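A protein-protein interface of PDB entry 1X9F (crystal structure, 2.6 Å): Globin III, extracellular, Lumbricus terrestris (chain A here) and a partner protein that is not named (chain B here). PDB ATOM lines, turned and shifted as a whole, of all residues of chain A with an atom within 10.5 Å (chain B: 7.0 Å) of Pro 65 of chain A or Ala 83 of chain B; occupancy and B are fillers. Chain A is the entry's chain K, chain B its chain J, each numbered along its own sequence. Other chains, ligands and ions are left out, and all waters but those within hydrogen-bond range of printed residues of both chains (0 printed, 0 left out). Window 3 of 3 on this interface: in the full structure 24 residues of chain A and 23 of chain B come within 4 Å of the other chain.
The side-chain amino group (NZ) of Lys 66 of chain A lies within salt-bridge range of the side-chain carboxylate (OE2) of Glu 87 of chain B (3.8 Å). NH1 of Arg 73 of chain A lies within salt-bridge range of OE1 of Glu 88 of chain B (3.0 Å).
Among the printed residues, pairs that only touch across the chains: Pro 65 of chain A with Ala 83 of chain B, Leu 72 of chain A with Thr 78 of chain B, Pro 65 of chain A with Glu 87 of chain B, Ile 33 of chain A with Gln 81 of chain B, Pro 65 of chain A with Thr 84 of chain B, Ser 68 of chain A with Thr 84 of chain B and Ala 69 of chain A with Thr 84 of chain B.
Of the 20 printed residues of chain A, 7 touch a printed residue of chain B. Printed residues of chain A that touch a printed residue of chain B: Ile 33, Pro 65, Lys 66, Ser 68, Ala 69, Leu 72 and Arg 73. Hydrophobic or aromatic side chains of chain A that line the printed part of chain B: Ile 33, Pro 65 and Leu 72. Of the 10 printed residues of chain B, 6 touch a printed residue of chain A. Printed residues of chain B that touch a printed residue of chain A: Thr 78, Gln 81, Ala 83, Thr 84, Glu 87 and Glu 88. Hydrophobic or aromatic side chains of chain B that line the printed part of chain A: Ala 83. Among the printed residues, 9 pairs touch across the chains. Among the printed residues, Asp or Glu carboxylates within 4 Å of a Lys or Arg side-chain nitrogen of the other chain: Lys 66 of chain A with Glu 87 of chain B and Arg 73 of chain A with Glu 88 of chain B.
The side-chain carboxylate (OD1) of Asp 80 of chain B is in hydrogen-bond range of the side-chain amide nitrogen (NE2) of Gln 81 of chain B. The backbone carbonyl oxygen (O) of Gly 64 of chain A sits at hydrogen-bond distance from the side-chain hydroxyl (OG) of Ser 68 of chain A (2.8 Å).
Of the printed residues of chain B, Ile 33 of chain A touches Gln 81. Pro 65 of chain A touches three residues of chain B. Printed residues of chain B within 4 Å of Ser 68 of chain A: Thr 84 (3.9 Å). Of the printed residues of chain B, Ala 69 of chain A touches Thr 84 (3.98 Å). Printed residues of chain B within 4 Å of Leu 72 of chain A: Thr 78 (3.6 Å). Of the printed residues of chain A, Gln 81 of chain B touches Ile 33. Pro 82 of chain B touches none of the printed residues of chain A. Ala 83 of chain B touches just one residue of chain A: Pro 65 (3.5 Å). The nearest residue of chain B that does not touch Pro 65 of chain A is Glu 88 of chain B (5.8 Å). The nearest residue of chain A that does not touch Ala 83 of chain B is Lys 66 of chain A (5.8 Å).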
ATOM      1  N   ILE A  33      22.304   1.568  15.282  1.00  0.00           N
ATOM      2  CA  ILE A  33      22.701   2.902  15.739  1.00  0.00           C
ATOM      3  C   ILE A  33      23.544   3.616  14.690  1.00  0.00           C
ATOM      4  O   ILE A  33      23.219   4.737  14.303  1.00  0.00           O
ATOM      5  CB  ILE A  33      23.427   2.854  17.113  1.00  0.00           C
ATOM      6  CG1 ILE A  33      22.465   2.405  18.215  1.00  0.00           C
ATOM      7  CG2 ILE A  33      23.988   4.230  17.482  1.00  0.00           C
ATOM      8  CD1 ILE A  33      23.148   1.882  19.473  1.00  0.00           C
ATOM      9  N   ARG A  37      21.731   6.714  12.809  1.00  0.00           N
ATOM     10  CA  ARG A  37      22.383   7.986  13.078  1.00  0.00           C
ATOM     11  C   ARG A  37      22.838   8.641  11.778  1.00  0.00           C
ATOM     12  O   ARG A  37      22.577   9.824  11.558  1.00  0.00           O
ATOM     13  CB  ARG A  37      23.571   7.758  14.016  1.00  0.00           C
ATOM     14  CG  ARG A  37      24.210   9.025  14.553  1.00  0.00           C
ATOM     15  CD  ARG A  37      25.450   9.421  13.773  1.00  0.00           C
ATOM     16  NE  ARG A  37      26.476  10.007  14.625  1.00  0.00           N
ATOM     17  CZ  ARG A  37      27.061   9.384  15.643  1.00  0.00           C
ATOM     18  NH1 ARG A  37      26.717   8.140  15.979  1.00  0.00           N
ATOM     19  NH2 ARG A  37      27.995  10.014  16.339  1.00  0.00           N
ATOM     20  N   ARG A  56      14.353  17.073  21.108  1.00  0.00           N
ATOM     21  CA  ARG A  56      13.950  16.186  22.201  1.00  0.00           C
ATOM     22  C   ARG A  56      14.807  14.905  22.322  1.00  0.00           C
ATOM     23  O   ARG A  56      14.981  14.377  23.426  1.00  0.00           O
ATOM     24  CB  ARG A  56      12.464  15.825  22.029  1.00  0.00           C
ATOM     25  CG  ARG A  56      11.694  15.562  23.326  1.00  0.00           C
ATOM     26  CD  ARG A  56      11.959  14.197  23.962  1.00  0.00           C
ATOM     27  NE  ARG A  56      11.049  13.143  23.504  1.00  0.00           N
ATOM     28  CZ  ARG A  56      11.304  11.834  23.567  1.00  0.00           C
ATOM     29  NH1 ARG A  56      12.465  11.389  24.055  1.00  0.00           N
ATOM     30  NH2 ARG A  56      10.398  10.965  23.126  1.00  0.00           N
ATOM     31  N   VAL A  57      15.335  14.412  21.198  1.00  0.00           N
ATOM     32  CA  VAL A  57      16.162  13.190  21.228  1.00  0.00           C
ATOM     33  C   VAL A  57      17.656  13.498  21.197  1.00  0.00           C
ATOM     34  O   VAL A  57      18.489  12.596  21.076  1.00  0.00           O
ATOM     35  CB  VAL A  57      15.769  12.156  20.129  1.00  0.00           C
ATOM     36  CG1 VAL A  57      14.434  11.502  20.466  1.00  0.00           C
ATOM     37  CG2 VAL A  57      15.746  12.788  18.738  1.00  0.00           C
ATOM     38  N   ASP A  58      17.973  14.786  21.334  1.00  0.00           N
ATOM     39  CA  ASP A  58      19.345  15.255  21.484  1.00  0.00           C
ATOM     40  C   ASP A  58      20.191  14.899  20.257  1.00  0.00           C
ATOM     41  O   ASP A  58      21.256  14.288  20.383  1.00  0.00           O
ATOM     42  CB  ASP A  58      19.966  14.715  22.796  1.00  0.00           C
ATOM     43  CG  ASP A  58      21.314  15.356  23.134  1.00  0.00           C
ATOM     44  OD1 ASP A  58      21.519  16.547  22.812  1.00  0.00           O
ATOM     45  OD2 ASP A  58      22.226  14.744  23.732  1.00  0.00           O
ATOM     46  N   ILE A  59      19.708  15.275  19.073  1.00  0.00           N
ATOM     47  CA  ILE A  59      20.484  15.112  17.834  1.00  0.00           C
ATOM     48  C   ILE A  59      21.807  15.879  17.910  1.00  0.00           C
ATOM     49  O   ILE A  59      22.806  15.488  17.302  1.00  0.00           O
ATOM     50  CB  ILE A  59      19.655  15.542  16.592  1.00  0.00           C
ATOM     51  CG1 ILE A  59      20.385  15.177  15.291  1.00  0.00           C
ATOM     52  CG2 ILE A  59      19.300  17.034  16.647  1.00  0.00           C
ATOM     53  CD1 ILE A  59      19.483  15.098  14.069  1.00  0.00           C
ATOM     54  N   GLU A  60      21.789  16.961  18.686  1.00  0.00           N
ATOM     55  CA  GLU A  60      22.946  17.808  18.956  1.00  0.00           C
ATOM     56  C   GLU A  60      24.185  16.993  19.326  1.00  0.00           C
ATOM     57  O   GLU A  60      25.310  17.352  18.967  1.00  0.00           O
ATOM     58  CB  GLU A  60      22.592  18.757  20.101  1.00  0.00           C
ATOM     59  CG  GLU A  60      23.459  20.000  20.212  1.00  0.00           C
ATOM     60  CD  GLU A  60      23.140  20.824  21.450  1.00  0.00           C
ATOM     61  OE1 GLU A  60      24.047  21.532  21.935  1.00  0.00           O
ATOM     62  OE2 GLU A  60      21.990  20.765  21.944  1.00  0.00           O
ATOM     63  N   HIS A  61      23.959  15.902  20.051  1.00  0.00           N
ATOM     64  CA  HIS A  61      25.001  14.955  20.410  1.00  0.00           C
ATOM     65  C   HIS A  61      24.611  13.616  19.812  1.00  0.00           C
ATOM     66  O   HIS A  61      24.219  12.695  20.534  1.00  0.00           O
ATOM     67  CB  HIS A  61      25.118  14.850  21.930  1.00  0.00           C
ATOM     68  CG  HIS A  61      25.235  16.175  22.609  1.00  0.00           C
ATOM     69  ND1 HIS A  61      24.175  17.049  22.715  1.00  0.00           N
ATOM     70  CD2 HIS A  61      26.287  16.785  23.202  1.00  0.00           C
ATOM     71  CE1 HIS A  61      24.568  18.142  23.343  1.00  0.00           C
ATOM     72  NE2 HIS A  61      25.845  18.007  23.652  1.00  0.00           N
ATOM     73  N   ALA A  62      24.700  13.527  18.483  1.00  0.00           N
ATOM     74  CA  ALA A  62      24.286  12.338  17.727  1.00  0.00           C
ATOM     75  C   ALA A  62      24.808  11.024  18.317  1.00  0.00           C
ATOM     76  O   ALA A  62      24.109  10.006  18.298  1.00  0.00           O
ATOM     77  CB  ALA A  62      24.695  12.472  16.264  1.00  0.00           C
ATOM     78  N   GLU A  63      26.025  11.066  18.856  1.00  0.00           N
ATOM     79  CA  GLU A  63      26.660   9.908  19.490  1.00  0.00           C
ATOM     80  C   GLU A  63      26.158   9.607  20.911  1.00  0.00           C
ATOM     81  O   GLU A  63      26.487   8.559  21.473  1.00  0.00           O
ATOM     82  CB  GLU A  63      28.185  10.091  19.516  1.00  0.00           C
ATOM     83  CG  GLU A  63      28.705  11.099  20.545  1.00  0.00           C
ATOM     84  CD  GLU A  63      28.351  12.545  20.221  1.00  0.00           C
ATOM     85  OE1 GLU A  63      28.505  12.958  19.050  1.00  0.00           O
ATOM     86  OE2 GLU A  63      27.928  13.278  21.143  1.00  0.00           O
ATOM     87  N   GLY A  64      25.380  10.522  21.492  1.00  0.00           N
ATOM     88  CA  GLY A  64      24.923  10.388  22.886  1.00  0.00           C
ATOM     89  C   GLY A  64      23.901   9.276  23.074  1.00  0.00           C
ATOM     90  O   GLY A  64      23.332   8.802  22.090  1.00  0.00           O
ATOM     91  N   PRO A  65      23.650   8.852  24.317  1.00  0.00           N
ATOM     92  CA  PRO A  65      22.694   7.762  24.562  1.00  0.00           C
ATOM     93  C   PRO A  65      21.249   8.129  24.184  1.00  0.00           C
ATOM     94  O   PRO A  65      20.495   7.254  23.751  1.00  0.00           O
ATOM     95  CB  PRO A  65      22.826   7.503  26.067  1.00  0.00           C
ATOM     96  CG  PRO A  65      23.313   8.811  26.631  1.00  0.00           C
ATOM     97  CD  PRO A  65      24.226   9.373  25.572  1.00  0.00           C
ATOM     98  N   LYS A  66      20.878   9.404  24.342  1.00  0.00           N
ATOM     99  CA  LYS A  66      19.560   9.908  23.920  1.00  0.00           C
ATOM    100  C   LYS A  66      19.237   9.616  22.454  1.00  0.00           C
ATOM    101  O   LYS A  66      18.212   8.998  22.144  1.00  0.00           O
ATOM    102  CB  LYS A  66      19.456  11.418  24.169  1.00  0.00           C
ATOM    103  CG  LYS A  66      18.929  11.806  25.542  1.00  0.00           C
ATOM    104  CD  LYS A  66      17.407  11.973  25.534  1.00  0.00           C
ATOM    105  CE  LYS A  66      16.831  12.114  26.943  1.00  0.00           C
ATOM    106  NZ  LYS A  66      17.501  13.166  27.770  1.00  0.00           N
ATOM    107  N   PHE A  67      20.120  10.068  21.564  1.00  0.00           N
ATOM    108  CA  PHE A  67      19.904   9.944  20.127  1.00  0.00           C
ATOM    109  C   PHE A  67      20.122   8.519  19.653  1.00  0.00           C
ATOM    110  O   PHE A  67      19.503   8.078  18.678  1.00  0.00           O
ATOM    111  CB  PHE A  67      20.812  10.902  19.354  1.00  0.00           C
ATOM    112  CG  PHE A  67      20.380  11.129  17.931  1.00  0.00           C
ATOM    113  CD1 PHE A  67      19.194  11.810  17.648  1.00  0.00           C
ATOM    114  CD2 PHE A  67      21.153  10.665  16.869  1.00  0.00           C
ATOM    115  CE1 PHE A  67      18.782  12.025  16.328  1.00  0.00           C
ATOM    116  CE2 PHE A  67      20.753  10.878  15.543  1.00  0.00           C
ATOM    117  CZ  PHE A  67      19.564  11.560  15.274  1.00  0.00           C
ATOM    118  N   SER A  68      21.008   7.809  20.353  1.00  0.00           N
ATOM    119  CA  SER A  68      21.284   6.411  20.058  1.00  0.00           C
ATOM    120  C   SER A  68      20.010   5.599  20.201  1.00  0.00           C
ATOM    121  O   SER A  68      19.650   4.833  19.304  1.00  0.00           O
ATOM    122  CB  SER A  68      22.372   5.864  20.983  1.00  0.00           C
ATOM    123  OG  SER A  68      23.647   6.387  20.622  1.00  0.00           O
ATOM    124  N   ALA A  69      19.320   5.787  21.324  1.00  0.00           N
ATOM    125  CA  ALA A  69      18.073   5.082  21.587  1.00  0.00           C
ATOM    126  C   ALA A  69      17.063   5.387  20.498  1.00  0.00           C
ATOM    127  O   ALA A  69      16.369   4.493  20.011  1.00  0.00           O
ATOM    128  CB  ALA A  69      17.518   5.468  22.951  1.00  0.00           C
ATOM    129  N   HIS A  70      16.996   6.660  20.118  1.00  0.00           N
ATOM    130  CA  HIS A  70      16.081   7.095  19.085  1.00  0.00           C
ATOM    131  C   HIS A  70      16.407   6.472  17.724  1.00  0.00           C
ATOM    132  O   HIS A  70      15.502   6.066  16.994  1.00  0.00           O
ATOM    133  CB  HIS A  70      16.085   8.609  18.971  1.00  0.00           C
ATOM    134  CG  HIS A  70      15.297   9.100  17.807  1.00  0.00           C
ATOM    135  ND1 HIS A  70      13.920   9.092  17.794  1.00  0.00           N
ATOM    136  CD2 HIS A  70      15.686   9.552  16.592  1.00  0.00           C
ATOM    137  CE1 HIS A  70      13.494   9.551  16.633  1.00  0.00           C
ATOM    138  NE2 HIS A  70      14.546   9.840  15.887  1.00  0.00           N
ATOM    139  N   ALA A  71      17.700   6.405  17.399  1.00  0.00           N
ATOM    140  CA  ALA A  71      18.184   5.778  16.166  1.00  0.00           C
ATOM    141  C   ALA A  71      17.714   4.331  16.092  1.00  0.00           C
ATOM    142  O   ALA A  71      17.303   3.848  15.027  1.00  0.00           O
ATOM    143  CB  ALA A  71      19.705   5.848  16.096  1.00  0.00           C
ATOM    144  N   LEU A  72      17.772   3.648  17.235  1.00  0.00           N
ATOM    145  CA  LEU A  72      17.240   2.296  17.353  1.00  0.00           C
ATOM    146  C   LEU A  72      15.732   2.273  17.160  1.00  0.00           C
ATOM    147  O   LEU A  72      15.214   1.385  16.486  1.00  0.00           O
ATOM    148  CB  LEU A  72      17.591   1.679  18.708  1.00  0.00           C
ATOM    149  CG  LEU A  72      19.071   1.398  18.960  1.00  0.00           C
ATOM    150  CD1 LEU A  72      19.306   1.211  20.445  1.00  0.00           C
ATOM    151  CD2 LEU A  72      19.543   0.182  18.177  1.00  0.00           C
ATOM    152  N   ARG A  73      15.032   3.240  17.744  1.00  0.00           N
ATOM    153  CA  ARG A  73      13.572   3.254  17.690  1.00  0.00           C
ATOM    154  C   ARG A  73      13.090   3.355  16.242  1.00  0.00           C
ATOM    155  O   ARG A  73      12.202   2.605  15.823  1.00  0.00           O
ATOM    156  CB  ARG A  73      13.031   4.405  18.533  1.00  0.00           C
ATOM    157  CG  ARG A  73      11.947   4.012  19.527  1.00  0.00           C
ATOM    158  CD  ARG A  73      12.196   4.553  20.933  1.00  0.00           C
ATOM    159  NE  ARG A  73      12.541   5.974  20.932  1.00  0.00           N
ATOM    160  CZ  ARG A  73      13.363   6.554  21.799  1.00  0.00           C
ATOM    161  NH1 ARG A  73      13.952   5.843  22.755  1.00  0.00           N
ATOM    162  NH2 ARG A  73      13.608   7.854  21.703  1.00  0.00           N
ATOM    163  N   THR B  78      20.645  -3.665  23.883  1.00  0.00           N
ATOM    164  CA  THR B  78      21.525  -2.695  24.546  1.00  0.00           C
ATOM    165  C   THR B  78      21.791  -3.017  26.016  1.00  0.00           C
ATOM    166  O   THR B  78      22.212  -2.136  26.774  1.00  0.00           O
ATOM    167  CB  THR B  78      20.977  -1.251  24.423  1.00  0.00           C
ATOM    168  OG1 THR B  78      19.647  -1.188  24.966  1.00  0.00           O
ATOM    169  CG2 THR B  78      20.802  -0.844  22.968  1.00  0.00           C
ATOM    170  N   ASP B  80      24.216  -4.431  27.120  1.00  0.00           N
ATOM    171  CA  ASP B  80      25.635  -4.117  27.305  1.00  0.00           C
ATOM    172  C   ASP B  80      25.988  -2.644  27.114  1.00  0.00           C
ATOM    173  O   ASP B  80      27.168  -2.278  27.160  1.00  0.00           O
ATOM    174  CB  ASP B  80      26.483  -4.940  26.337  1.00  0.00           C
ATOM    175  CG  ASP B  80      26.217  -4.573  24.877  1.00  0.00           C
ATOM    176  OD1 ASP B  80      25.032  -4.419  24.490  1.00  0.00           O
ATOM    177  OD2 ASP B  80      27.131  -4.428  24.038  1.00  0.00           O
ATOM    178  N   GLN B  81      24.987  -1.802  26.875  1.00  0.00           N
ATOM    179  CA  GLN B  81      25.222  -0.364  26.765  1.00  0.00           C
ATOM    180  C   GLN B  81      24.261   0.327  27.723  1.00  0.00           C
ATOM    181  O   GLN B  81      23.191   0.800  27.314  1.00  0.00           O
ATOM    182  CB  GLN B  81      25.017   0.124  25.329  1.00  0.00           C
ATOM    183  CG  GLN B  81      25.756  -0.692  24.274  1.00  0.00           C
ATOM    184  CD  GLN B  81      25.062  -0.656  22.927  1.00  0.00           C
ATOM    185  OE1 GLN B  81      24.914   0.409  22.326  1.00  0.00           O
ATOM    186  NE2 GLN B  81      24.632  -1.819  22.446  1.00  0.00           N
ATOM    187  N   PRO B  82      24.644   0.364  29.002  1.00  0.00           N
ATOM    188  CA  PRO B  82      23.770   0.847  30.077  1.00  0.00           C
ATOM    189  C   PRO B  82      23.141   2.222  29.828  1.00  0.00           C
ATOM    190  O   PRO B  82      21.952   2.404  30.101  1.00  0.00           O
ATOM    191  CB  PRO B  82      24.700   0.894  31.302  1.00  0.00           C
ATOM    192  CG  PRO B  82      26.082   0.758  30.760  1.00  0.00           C
ATOM    193  CD  PRO B  82      25.955  -0.069  29.524  1.00  0.00           C
ATOM    194  N   ALA B  83      23.921   3.171  29.318  1.00  0.00           N
ATOM    195  CA  ALA B  83      23.422   4.533  29.142  1.00  0.00           C
ATOM    196  C   ALA B  83      22.308   4.596  28.099  1.00  0.00           C
ATOM    197  O   ALA B  83      21.284   5.256  28.311  1.00  0.00           O
ATOM    198  CB  ALA B  83      24.559   5.480  28.786  1.00  0.00           C
ATOM    199  N   THR B  84      22.520   3.905  26.981  1.00  0.00           N
ATOM    200  CA  THR B  84      21.520   3.793  25.925  1.00  0.00           C
ATOM    201  C   THR B  84      20.308   3.029  26.435  1.00  0.00           C
ATOM    202  O   THR B  84      19.169   3.436  26.191  1.00  0.00           O
ATOM    203  CB  THR B  84      22.107   3.065  24.705  1.00  0.00           C
ATOM    204  OG1 THR B  84      23.183   3.838  24.159  1.00  0.00           O
ATOM    205  CG2 THR B  84      21.097   3.006  23.557  1.00  0.00           C
ATOM    206  N   LEU B  85      20.549   1.924  27.138  1.00  0.00           N
ATOM    207  CA  LEU B  85      19.450   1.126  27.674  1.00  0.00           C
ATOM    208  C   LEU B  85      18.558   1.981  28.571  1.00  0.00           C
ATOM    209  O   LEU B  85      17.330   1.889  28.512  1.00  0.00           O
ATOM    210  CB  LEU B  85      19.972  -0.091  28.449  1.00  0.00           C
ATOM    211  CG  LEU B  85      18.941  -0.954  29.196  1.00  0.00           C
ATOM    212  CD1 LEU B  85      17.928  -1.598  28.250  1.00  0.00           C
ATOM    213  CD2 LEU B  85      19.630  -2.022  30.038  1.00  0.00           C
ATOM    214  N   LYS B  86      19.201   2.813  29.391  1.00  0.00           N
ATOM    215  CA  LYS B  86      18.513   3.683  30.335  1.00  0.00           C
ATOM    216  C   LYS B  86      17.611   4.633  29.575  1.00  0.00           C
ATOM    217  O   LYS B  86      16.440   4.820  29.928  1.00  0.00           O
ATOM    218  CB  LYS B  86      19.545   4.475  31.148  1.00  0.00           C
ATOM    219  CG  LYS B  86      18.972   5.311  32.283  1.00  0.00           C
ATOM    220  CD  LYS B  86      18.369   4.441  33.382  1.00  0.00           C
ATOM    221  CE  LYS B  86      17.903   5.278  34.566  1.00  0.00           C
ATOM    222  NZ  LYS B  86      16.868   6.301  34.189  1.00  0.00           N
ATOM    223  N   GLU B  87      18.165   5.217  28.518  1.00  0.00           N
ATOM    224  CA  GLU B  87      17.418   6.143  27.695  1.00  0.00           C
ATOM    225  C   GLU B  87      16.224   5.464  27.028  1.00  0.00           C
ATOM    226  O   GLU B  87      15.148   6.057  26.930  1.00  0.00           O
ATOM    227  CB  GLU B  87      18.340   6.795  26.669  1.00  0.00           C
ATOM    228  CG  GLU B  87      18.298   8.313  26.714  1.00  0.00           C
ATOM    229  CD  GLU B  87      18.375   8.866  28.128  1.00  0.00           C
ATOM    230  OE1 GLU B  87      19.422   8.694  28.796  1.00  0.00           O
ATOM    231  OE2 GLU B  87      17.374   9.473  28.580  1.00  0.00           O
ATOM    232  N   GLU B  88      16.400   4.222  26.586  1.00  0.00           N
ATOM    233  CA  GLU B  88      15.286   3.505  25.978  1.00  0.00           C
ATOM    234  C   GLU B  88      14.243   3.144  27.024  1.00  0.00           C
ATOM    235  O   GLU B  88      13.048   3.348  26.802  1.00  0.00           O
ATOM    236  CB  GLU B  88      15.755   2.254  25.227  1.00  0.00           C
ATOM    237  CG  GLU B  88      14.624   1.304  24.829  1.00  0.00           C
ATOM    238  CD  GLU B  88      13.633   1.901  23.835  1.00  0.00           C
ATOM    239  OE1 GLU B  88      13.960   2.910  23.168  1.00  0.00           O
ATOM    240  OE2 GLU B  88      12.518   1.349  23.717  1.00  0.00           O
